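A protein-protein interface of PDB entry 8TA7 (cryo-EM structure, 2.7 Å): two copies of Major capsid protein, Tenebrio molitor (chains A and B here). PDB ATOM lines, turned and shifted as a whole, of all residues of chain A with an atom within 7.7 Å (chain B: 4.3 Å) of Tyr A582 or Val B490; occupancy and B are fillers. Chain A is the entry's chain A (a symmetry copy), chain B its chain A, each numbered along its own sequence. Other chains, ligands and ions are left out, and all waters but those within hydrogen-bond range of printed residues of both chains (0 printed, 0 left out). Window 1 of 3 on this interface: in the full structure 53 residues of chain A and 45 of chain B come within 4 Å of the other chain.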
ATOM      1  N   SER A 287      -9.183   3.652   6.942  1.00  0.00           N
ATOM      2  CA  SER A 287      -8.116   4.145   7.801  1.00  0.00           C
ATOM      3  C   SER A 287      -6.829   3.336   7.689  1.00  0.00           C
ATOM      4  O   SER A 287      -5.825   3.713   8.300  1.00  0.00           O
ATOM      5  CB  SER A 287      -8.581   4.158   9.258  1.00  0.00           C
ATOM      6  OG  SER A 287      -8.838   2.845   9.723  1.00  0.00           O
ATOM      7  N   ILE A 288      -6.833   2.243   6.934  1.00  0.00           N
ATOM      8  CA  ILE A 288      -5.641   1.413   6.772  1.00  0.00           C
ATOM      9  C   ILE A 288      -4.617   2.171   5.935  1.00  0.00           C
ATOM     10  O   ILE A 288      -4.941   2.637   4.833  1.00  0.00           O
ATOM     11  CB  ILE A 288      -5.991   0.055   6.147  1.00  0.00           C
ATOM     12  CG1 ILE A 288      -6.896  -0.737   7.091  1.00  0.00           C
ATOM     13  CG2 ILE A 288      -4.732  -0.725   5.837  1.00  0.00           C
ATOM     14  CD1 ILE A 288      -7.362  -2.051   6.529  1.00  0.00           C
ATOM     15  N   PRO A 289      -3.377   2.320   6.416  1.00  0.00           N
ATOM     16  CA  PRO A 289      -2.433   3.212   5.723  1.00  0.00           C
ATOM     17  C   PRO A 289      -1.969   2.691   4.376  1.00  0.00           C
ATOM     18  O   PRO A 289      -1.905   3.459   3.409  1.00  0.00           O
ATOM     19  CB  PRO A 289      -1.265   3.320   6.715  1.00  0.00           C
ATOM     20  CG  PRO A 289      -1.816   2.870   8.026  1.00  0.00           C
ATOM     21  CD  PRO A 289      -2.845   1.843   7.699  1.00  0.00           C
ATOM     22  N   PHE A 290      -1.634   1.409   4.284  1.00  0.00           N
ATOM     23  CA  PHE A 290      -1.031   0.851   3.082  1.00  0.00           C
ATOM     24  C   PHE A 290      -2.047   0.469   2.015  1.00  0.00           C
ATOM     25  O   PHE A 290      -1.650   0.195   0.879  1.00  0.00           O
ATOM     26  CB  PHE A 290      -0.184  -0.370   3.445  1.00  0.00           C
ATOM     27  CG  PHE A 290      -0.906  -1.368   4.296  1.00  0.00           C
ATOM     28  CD1 PHE A 290      -1.618  -2.403   3.719  1.00  0.00           C
ATOM     29  CD2 PHE A 290      -0.881  -1.266   5.675  1.00  0.00           C
ATOM     30  CE1 PHE A 290      -2.284  -3.314   4.502  1.00  0.00           C
ATOM     31  CE2 PHE A 290      -1.546  -2.174   6.459  1.00  0.00           C
ATOM     32  CZ  PHE A 290      -2.252  -3.195   5.874  1.00  0.00           C
ATOM     33  N   LYS A 439      -0.884  19.490  10.519  1.00  0.00           N
ATOM     34  CA  LYS A 439       0.258  18.718  10.047  1.00  0.00           C
ATOM     35  C   LYS A 439       0.104  18.438   8.558  1.00  0.00           C
ATOM     36  O   LYS A 439      -0.902  17.867   8.127  1.00  0.00           O
ATOM     37  CB  LYS A 439       0.401  17.409  10.820  1.00  0.00           C
ATOM     38  CG  LYS A 439       1.634  16.614  10.421  1.00  0.00           C
ATOM     39  CD  LYS A 439       1.872  15.433  11.339  1.00  0.00           C
ATOM     40  CE  LYS A 439       3.102  14.652  10.909  1.00  0.00           C
ATOM     41  NZ  LYS A 439       3.412  13.534  11.836  1.00  0.00           N
ATOM     42  N   THR A 440       1.102  18.841   7.780  1.00  0.00           N
ATOM     43  CA  THR A 440       1.166  18.550   6.357  1.00  0.00           C
ATOM     44  C   THR A 440       2.227  17.489   6.103  1.00  0.00           C
ATOM     45  O   THR A 440       3.363  17.612   6.566  1.00  0.00           O
ATOM     46  CB  THR A 440       1.489  19.810   5.552  1.00  0.00           C
ATOM     47  OG1 THR A 440       0.496  20.809   5.809  1.00  0.00           O
ATOM     48  CG2 THR A 440       1.512  19.498   4.067  1.00  0.00           C
ATOM     49  N   THR A 441       1.853  16.449   5.363  1.00  0.00           N
ATOM     50  CA  THR A 441       2.774  15.371   5.041  1.00  0.00           C
ATOM     51  C   THR A 441       3.000  15.339   3.539  1.00  0.00           C
ATOM     52  O   THR A 441       2.321  16.022   2.770  1.00  0.00           O
ATOM     53  CB  THR A 441       2.260  14.005   5.521  1.00  0.00           C
ATOM     54  OG1 THR A 441       0.996  13.725   4.905  1.00  0.00           O
ATOM     55  CG2 THR A 441       2.103  13.992   7.030  1.00  0.00           C
ATOM     56  N   ASP A 442       3.980  14.535   3.133  1.00  0.00           N
ATOM     57  CA  ASP A 442       4.331  14.398   1.723  1.00  0.00           C
ATOM     58  C   ASP A 442       4.710  12.938   1.500  1.00  0.00           C
ATOM     59  O   ASP A 442       5.823  12.526   1.841  1.00  0.00           O
ATOM     60  CB  ASP A 442       5.465  15.344   1.348  1.00  0.00           C
ATOM     61  CG  ASP A 442       5.786  15.316  -0.128  1.00  0.00           C
ATOM     62  OD1 ASP A 442       5.072  14.633  -0.883  1.00  0.00           O
ATOM     63  OD2 ASP A 442       6.754  15.989  -0.537  1.00  0.00           O
ATOM     64  N   SER A 443       3.781  12.164   0.936  1.00  0.00           N
ATOM     65  CA  SER A 443       4.033  10.749   0.702  1.00  0.00           C
ATOM     66  C   SER A 443       5.044  10.510  -0.412  1.00  0.00           C
ATOM     67  O   SER A 443       5.594   9.407  -0.496  1.00  0.00           O
ATOM     68  CB  SER A 443       2.723  10.031   0.383  1.00  0.00           C
ATOM     69  OG  SER A 443       2.850   8.638   0.604  1.00  0.00           O
ATOM     70  N   SER A 444       5.297  11.506  -1.259  1.00  0.00           N
ATOM     71  CA  SER A 444       6.378  11.431  -2.229  1.00  0.00           C
ATOM     72  C   SER A 444       7.747  11.607  -1.590  1.00  0.00           C
ATOM     73  O   SER A 444       8.759  11.409  -2.270  1.00  0.00           O
ATOM     74  CB  SER A 444       6.182  12.485  -3.320  1.00  0.00           C
ATOM     75  OG  SER A 444       6.579  13.768  -2.871  1.00  0.00           O
ATOM     76  N   GLN A 445       7.793  11.982  -0.311  1.00  0.00           N
ATOM     77  CA  GLN A 445       9.023  12.188   0.449  1.00  0.00           C
ATOM     78  C   GLN A 445       9.920  13.254  -0.165  1.00  0.00           C
ATOM     79  O   GLN A 445      11.130  13.269   0.081  1.00  0.00           O
ATOM     80  CB  GLN A 445       9.799  10.879   0.626  1.00  0.00           C
ATOM     81  CG  GLN A 445       9.044   9.826   1.407  1.00  0.00           C
ATOM     82  CD  GLN A 445       9.939   8.707   1.880  1.00  0.00           C
ATOM     83  OE1 GLN A 445      11.123   8.670   1.556  1.00  0.00           O
ATOM     84  NE2 GLN A 445       9.379   7.787   2.654  1.00  0.00           N
ATOM     85  N   THR A 447       9.513  16.430   0.610  1.00  0.00           N
ATOM     86  CA  THR A 447       9.688  17.318   1.748  1.00  0.00           C
ATOM     87  C   THR A 447       9.326  16.584   3.031  1.00  0.00           C
ATOM     88  O   THR A 447       8.520  15.651   3.018  1.00  0.00           O
ATOM     89  CB  THR A 447       8.823  18.581   1.615  1.00  0.00           C
ATOM     90  OG1 THR A 447       7.442  18.211   1.521  1.00  0.00           O
ATOM     91  CG2 THR A 447       9.217  19.379   0.382  1.00  0.00           C
ATOM     92  N   ALA A 448       9.932  17.012   4.135  1.00  0.00           N
ATOM     93  CA  ALA A 448       9.621  16.439   5.434  1.00  0.00           C
ATOM     94  C   ALA A 448       8.249  16.917   5.909  1.00  0.00           C
ATOM     95  O   ALA A 448       7.746  17.943   5.442  1.00  0.00           O
ATOM     96  CB  ALA A 448      10.690  16.826   6.452  1.00  0.00           C
ATOM     97  N   PRO A 449       7.613  16.185   6.824  1.00  0.00           N
ATOM     98  CA  PRO A 449       6.344  16.662   7.386  1.00  0.00           C
ATOM     99  C   PRO A 449       6.535  17.968   8.143  1.00  0.00           C
ATOM    100  O   PRO A 449       7.593  18.228   8.719  1.00  0.00           O
ATOM    101  CB  PRO A 449       5.915  15.525   8.321  1.00  0.00           C
ATOM    102  CG  PRO A 449       6.657  14.333   7.840  1.00  0.00           C
ATOM    103  CD  PRO A 449       7.962  14.847   7.326  1.00  0.00           C
ATOM    104  N   GLN A 499     -11.650  10.475  13.397  1.00  0.00           N
ATOM    105  CA  GLN A 499     -11.972   9.716  12.200  1.00  0.00           C
ATOM    106  C   GLN A 499     -13.015   8.659  12.534  1.00  0.00           C
ATOM    107  O   GLN A 499     -12.802   7.835  13.425  1.00  0.00           O
ATOM    108  CB  GLN A 499     -10.718   9.061  11.617  1.00  0.00           C
ATOM    109  CG  GLN A 499     -10.938   8.351  10.308  1.00  0.00           C
ATOM    110  CD  GLN A 499      -9.664   7.744   9.767  1.00  0.00           C
ATOM    111  OE1 GLN A 499      -8.610   7.818  10.398  1.00  0.00           O
ATOM    112  NE2 GLN A 499      -9.755   7.131   8.596  1.00  0.00           N
ATOM    113  N   PRO A 579      -8.558   9.073  -0.459  1.00  0.00           N
ATOM    114  CA  PRO A 579      -7.815   8.036   0.263  1.00  0.00           C
ATOM    115  C   PRO A 579      -7.034   8.635   1.422  1.00  0.00           C
ATOM    116  O   PRO A 579      -6.671   9.813   1.412  1.00  0.00           O
ATOM    117  CB  PRO A 579      -6.884   7.454  -0.808  1.00  0.00           C
ATOM    118  CG  PRO A 579      -6.755   8.525  -1.819  1.00  0.00           C
ATOM    119  CD  PRO A 579      -8.070   9.239  -1.838  1.00  0.00           C
ATOM    120  N   ASN A 580      -6.785   7.808   2.432  1.00  0.00           N
ATOM    121  CA  ASN A 580      -6.122   8.288   3.635  1.00  0.00           C
ATOM    122  C   ASN A 580      -4.697   8.735   3.339  1.00  0.00           C
ATOM    123  O   ASN A 580      -4.072   8.312   2.363  1.00  0.00           O
ATOM    124  CB  ASN A 580      -6.151   7.211   4.731  1.00  0.00           C
ATOM    125  CG  ASN A 580      -5.375   5.948   4.368  1.00  0.00           C
ATOM    126  OD1 ASN A 580      -4.368   5.980   3.667  1.00  0.00           O
ATOM    127  ND2 ASN A 580      -5.862   4.817   4.852  1.00  0.00           N
ATOM    128  N   VAL A 581      -4.196   9.634   4.180  1.00  0.00           N
ATOM    129  CA  VAL A 581      -2.817  10.095   4.125  1.00  0.00           C
ATOM    130  C   VAL A 581      -2.137   9.673   5.420  1.00  0.00           C
ATOM    131  O   VAL A 581      -2.401  10.241   6.487  1.00  0.00           O
ATOM    132  CB  VAL A 581      -2.730  11.612   3.893  1.00  0.00           C
ATOM    133  CG1 VAL A 581      -3.052  11.928   2.451  1.00  0.00           C
ATOM    134  CG2 VAL A 581      -3.712  12.354   4.788  1.00  0.00           C
ATOM    135  N   TYR A 582      -1.273   8.663   5.325  1.00  0.00           N
ATOM    136  CA  TYR A 582      -0.607   8.080   6.486  1.00  0.00           C
ATOM    137  C   TYR A 582      -1.627   7.618   7.524  1.00  0.00           C
ATOM    138  O   TYR A 582      -1.435   7.771   8.730  1.00  0.00           O
ATOM    139  CB  TYR A 582       0.392   9.062   7.097  1.00  0.00           C
ATOM    140  CG  TYR A 582       1.616   9.292   6.243  1.00  0.00           C
ATOM    141  CD1 TYR A 582       1.665  10.339   5.336  1.00  0.00           C
ATOM    142  CD2 TYR A 582       2.716   8.455   6.335  1.00  0.00           C
ATOM    143  CE1 TYR A 582       2.779  10.553   4.552  1.00  0.00           C
ATOM    144  CE2 TYR A 582       3.835   8.661   5.555  1.00  0.00           C
ATOM    145  CZ  TYR A 582       3.860   9.712   4.666  1.00  0.00           C
ATOM    146  OH  TYR A 582       4.975   9.917   3.888  1.00  0.00           O
ATOM    147  N   GLY A 583      -2.729   7.048   7.041  1.00  0.00           N
ATOM    148  CA  GLY A 583      -3.790   6.567   7.899  1.00  0.00           C
ATOM    149  C   GLY A 583      -4.738   7.627   8.411  1.00  0.00           C
ATOM    150  O   GLY A 583      -5.558   7.326   9.287  1.00  0.00           O
ATOM    151  N   ARG A 584      -4.663   8.849   7.898  1.00  0.00           N
ATOM    152  CA  ARG A 584      -5.442   9.967   8.407  1.00  0.00           C
ATOM    153  C   ARG A 584      -6.384  10.501   7.339  1.00  0.00           C
ATOM    154  O   ARG A 584      -6.082  10.449   6.145  1.00  0.00           O
ATOM    155  CB  ARG A 584      -4.523  11.094   8.879  1.00  0.00           C
ATOM    156  CG  ARG A 584      -3.397  10.645   9.784  1.00  0.00           C
ATOM    157  CD  ARG A 584      -3.912  10.287  11.159  1.00  0.00           C
ATOM    158  NE  ARG A 584      -4.066  11.472  11.993  1.00  0.00           N
ATOM    159  CZ  ARG A 584      -3.115  11.967  12.776  1.00  0.00           C
ATOM    160  NH1 ARG A 584      -1.923  11.400  12.855  1.00  0.00           N
ATOM    161  NH2 ARG A 584      -3.367  13.058  13.491  1.00  0.00           N
ATOM    162  N   MET A 585      -7.531  11.010   7.779  1.00  0.00           N
ATOM    163  CA  MET A 585      -8.390  11.806   6.915  1.00  0.00           C
ATOM    164  C   MET A 585      -7.887  13.240   6.879  1.00  0.00           C
ATOM    165  O   MET A 585      -7.511  13.804   7.911  1.00  0.00           O
ATOM    166  CB  MET A 585      -9.839  11.752   7.392  1.00  0.00           C
ATOM    167  CG  MET A 585     -10.419  10.357   7.383  1.00  0.00           C
ATOM    168  SD  MET A 585     -10.552   9.730   5.699  1.00  0.00           S
ATOM    169  CE  MET A 585      -9.303   8.457   5.708  1.00  0.00           C
ATOM    170  N   TYR B 427      -3.627  17.329   7.487  1.00  0.00           N
ATOM    171  CA  TYR B 427      -4.630  16.858   8.430  1.00  0.00           C
ATOM    172  C   TYR B 427      -4.386  17.536   9.768  1.00  0.00           C
ATOM    173  O   TYR B 427      -3.242  17.893  10.076  1.00  0.00           O
ATOM    174  CB  TYR B 427      -4.598  15.328   8.573  1.00  0.00           C
ATOM    175  CG  TYR B 427      -3.235  14.746   8.854  1.00  0.00           C
ATOM    176  CD1 TYR B 427      -2.781  14.584  10.153  1.00  0.00           C
ATOM    177  CD2 TYR B 427      -2.406  14.346   7.816  1.00  0.00           C
ATOM    178  CE1 TYR B 427      -1.541  14.048  10.410  1.00  0.00           C
ATOM    179  CE2 TYR B 427      -1.164  13.810   8.063  1.00  0.00           C
ATOM    180  CZ  TYR B 427      -0.736  13.661   9.364  1.00  0.00           C
ATOM    181  OH  TYR B 427       0.504  13.125   9.619  1.00  0.00           O
ATOM    182  N   TYR B 459      14.101  11.760   5.227  1.00  0.00           N
ATOM    183  CA  TYR B 459      13.732  10.364   5.412  1.00  0.00           C
ATOM    184  C   TYR B 459      14.942   9.456   5.259  1.00  0.00           C
ATOM    185  O   TYR B 459      15.820   9.698   4.428  1.00  0.00           O
ATOM    186  CB  TYR B 459      12.661   9.966   4.400  1.00  0.00           C
ATOM    187  CG  TYR B 459      11.393  10.778   4.487  1.00  0.00           C
ATOM    188  CD1 TYR B 459      10.303  10.322   5.212  1.00  0.00           C
ATOM    189  CD2 TYR B 459      11.283  12.001   3.839  1.00  0.00           C
ATOM    190  CE1 TYR B 459       9.143  11.059   5.291  1.00  0.00           C
ATOM    191  CE2 TYR B 459      10.127  12.745   3.915  1.00  0.00           C
ATOM    192  CZ  TYR B 459       9.060  12.270   4.641  1.00  0.00           C
ATOM    193  OH  TYR B 459       7.904  13.009   4.718  1.00  0.00           O
ATOM    194  N   GLU B 489       9.271   9.546  13.503  1.00  0.00           N
ATOM    195  CA  GLU B 489       8.346   8.864  12.615  1.00  0.00           C
ATOM    196  C   GLU B 489       7.179   9.776  12.265  1.00  0.00           C
ATOM    197  O   GLU B 489       6.832  10.694  13.013  1.00  0.00           O
ATOM    198  CB  GLU B 489       7.815   7.583  13.254  1.00  0.00           C
ATOM    199  CG  GLU B 489       8.765   6.414  13.186  1.00  0.00           C
ATOM    200  CD  GLU B 489       8.226   5.192  13.899  1.00  0.00           C
ATOM    201  OE1 GLU B 489       7.079   5.245  14.388  1.00  0.00           O
ATOM    202  OE2 GLU B 489       8.953   4.179  13.974  1.00  0.00           O
ATOM    203  N   VAL B 490       6.566   9.510  11.109  1.00  0.00           N
ATOM    204  CA  VAL B 490       5.362  10.234  10.730  1.00  0.00           C
ATOM    205  C   VAL B 490       4.198   9.819  11.625  1.00  0.00           C
ATOM    206  O   VAL B 490       3.163  10.492  11.665  1.00  0.00           O
ATOM    207  CB  VAL B 490       5.082   9.997   9.231  1.00  0.00           C
ATOM    208  CG1 VAL B 490       3.782  10.651   8.786  1.00  0.00           C
ATOM    209  CG2 VAL B 490       6.252  10.477   8.388  1.00  0.00           C
ATOM    210  N   ASN B 491       4.375   8.745  12.393  1.00  0.00           N
ATOM    211  CA  ASN B 491       3.347   8.252  13.297  1.00  0.00           C
ATOM    212  C   ASN B 491       2.999   9.298  14.352  1.00  0.00           C
ATOM    213  O   ASN B 491       3.731  10.266  14.571  1.00  0.00           O
ATOM    214  CB  ASN B 491       3.835   6.965  13.968  1.00  0.00           C
ATOM    215  CG  ASN B 491       2.735   6.231  14.701  1.00  0.00           C
ATOM    216  OD1 ASN B 491       1.552   6.506  14.508  1.00  0.00           O
ATOM    217  ND2 ASN B 491       3.122   5.288  15.552  1.00  0.00           N
ATOM    218  N   VAL B 492       1.860   9.083  15.017  1.00  0.00           N
ATOM    219  CA  VAL B 492       1.392   9.969  16.077  1.00  0.00           C
ATOM    220  C   VAL B 492       2.198   9.807  17.359  1.00  0.00           C
ATOM    221  O   VAL B 492       2.053  10.611  18.286  1.00  0.00           O
ATOM    222  CB  VAL B 492      -0.114   9.689  16.294  1.00  0.00           C
ATOM    223  CG1 VAL B 492      -0.722  10.570  17.380  1.00  0.00           C
ATOM    224  CG2 VAL B 492      -0.872   9.838  14.988  1.00  0.00           C
ATOM    225  N   ASN B 557       3.264   3.224   5.523  1.00  0.00           N
ATOM    226  CA  ASN B 557       3.952   4.507   5.450  1.00  0.00           C
ATOM    227  C   ASN B 557       3.982   5.221   6.796  1.00  0.00           C
ATOM    228  O   ASN B 557       4.776   6.150   6.974  1.00  0.00           O
ATOM    229  CB  ASN B 557       3.308   5.386   4.374  1.00  0.00           C
ATOM    230  CG  ASN B 557       1.851   5.676   4.648  1.00  0.00           C
ATOM    231  OD1 ASN B 557       1.213   5.008   5.459  1.00  0.00           O
ATOM    232  ND2 ASN B 557       1.311   6.668   3.956  1.00  0.00           N
ATOM    233  N   THR B 558       3.155   4.793   7.752  1.00  0.00           N
ATOM    234  CA  THR B 558       3.259   5.312   9.111  1.00  0.00           C
ATOM    235  C   THR B 558       4.556   4.876   9.782  1.00  0.00           C
ATOM    236  O   THR B 558       4.927   5.422  10.826  1.00  0.00           O
ATOM    237  CB  THR B 558       2.058   4.859   9.941  1.00  0.00           C
ATOM    238  OG1 THR B 558       1.902   3.440   9.819  1.00  0.00           O
ATOM    239  CG2 THR B 558       0.792   5.541   9.460  1.00  0.00           C
ATOM    240  N   SER B 560       7.482   5.205   8.300  1.00  0.00           N
ATOM    241  CA  SER B 560       8.580   5.981   7.741  1.00  0.00           C
ATOM    242  C   SER B 560       9.309   6.739   8.843  1.00  0.00           C
ATOM    243  O   SER B 560       8.693   7.247   9.783  1.00  0.00           O
ATOM    244  CB  SER B 560       8.056   6.955   6.689  1.00  0.00           C
ATOM    245  OG  SER B 560       7.313   6.276   5.694  1.00  0.00           O
ATOM    246  N   LEU B 562      12.364   9.672   9.865  1.00  0.00           N
ATOM    247  CA  LEU B 562      13.154  10.827   9.474  1.00  0.00           C
ATOM    248  C   LEU B 562      14.244  11.080  10.503  1.00  0.00           C
ATOM    249  O   LEU B 562      14.073  10.817  11.696  1.00  0.00           O
ATOM    250  CB  LEU B 562      12.288  12.082   9.325  1.00  0.00           C
ATOM    251  CG  LEU B 562      11.206  12.044   8.249  1.00  0.00           C
ATOM    252  CD1 LEU B 562       9.839  11.797   8.863  1.00  0.00           C
ATOM    253  CD2 LEU B 562      11.223  13.328   7.444  1.00  0.00           C
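The backbone NH of Tyr B427 sits at hydrogen-bond distance from the backbone carbonyl oxygen of Lys A439, at 2.9 Å. O of Thr A447 is in hydrogen-bond range of OH of Tyr B459 (3.2 Å). NZ of Lys A439 lies within hydrogen-bond range of O of Val B490, at 3.1 Å.
The backbone NH (N) of Val B490 lies within hydrogen-bond range of the backbone carbonyl oxygen (O) of Ser B560 (3.4 Å). O of Asn B557 sits at hydrogen-bond distance from OG of Ser B560 (2.8 Å). OG of Ser A444 lies within hydrogen-bond range of OD1 of Asp A442, at 2.6 Å. The side-chain carboxylate of Asp A442 is in hydrogen-bond range of the backbone NH of Thr A447. The side-chain hydroxyl (OH) of Tyr A582 sits at hydrogen-bond distance from the backbone carbonyl oxygen (O) of Asp A442 (3.4 Å).
Among the printed residues, merely in contact across the chains: Pro A289 with Asn B557 (3.3 Å), Pro A289 with Thr B558 (3.999 Å), Thr A441 with Tyr B427 (3.2 Å), Asp A442 with Tyr B459 (3.6 Å), Gln A445 with Tyr B459 (3.5 Å), Gln A445 with Ser B560 (3.97 Å), Ala A448 with Tyr B459 (3.9 Å), Ala A448 with Leu B562 (3.7 Å), Pro A449 with Tyr B459 (3.2 Å), Pro A449 with Val B490 (3.9 Å), Pro A449 with Leu B562 (3.6 Å), Val A581 with Tyr B427 (3.9 Å), Tyr A582 with Val B490 (3.5 Å), Tyr A582 with Asn B557 (3.0 Å), Tyr A582 with Thr B558 (3.2 Å), Arg A584 with Tyr B427 (3.5 Å), Arg A584 with Val B492 (2.8 Å) and Met A585 with Tyr B427 (3.4 Å).
Ser A287 touches none of the printed residues of chain B. Thr A440 touches none of the printed residues of chain B. Printed residues of chain B within 4 Å of Thr A441: Tyr B427. Printed residues of chain B within 4 Å of Asp A442: Tyr B459 (3.6 Å). Tyr A582 touches just these residues of chain B: Val B490, Asn B557 and Thr B558. Printed residues of chain A within 4 Å of Tyr B427: Lys A439 (2.9 Å), Thr A441 (3.2 Å), Val A581 (3.9 Å), Arg A584 (3.5 Å) and Met A585 (3.4 Å). Of the printed residues of chain A, Thr B558 touches Pro A289 and Tyr A582. The nearest printed residue of chain B that does not touch Ala A448 is Val B490 (7.2 Å).
Of the 10 printed residues of chain B, 8 touch a printed residue of chain A. Hydrophobic or aromatic side chains of chain B within 4 Å of the printed part of chain A: Tyr B427, Tyr B459, Val B490, Val B492 and Leu B562. Along chain B the printed residues that touch a printed residue of chain A span positions 427 to 562. Among the printed residues, no Asp or Glu carboxylate lies within 4 Å of a Lys or Arg side-chain nitrogen of the other chain.
No position is printed for both chains.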
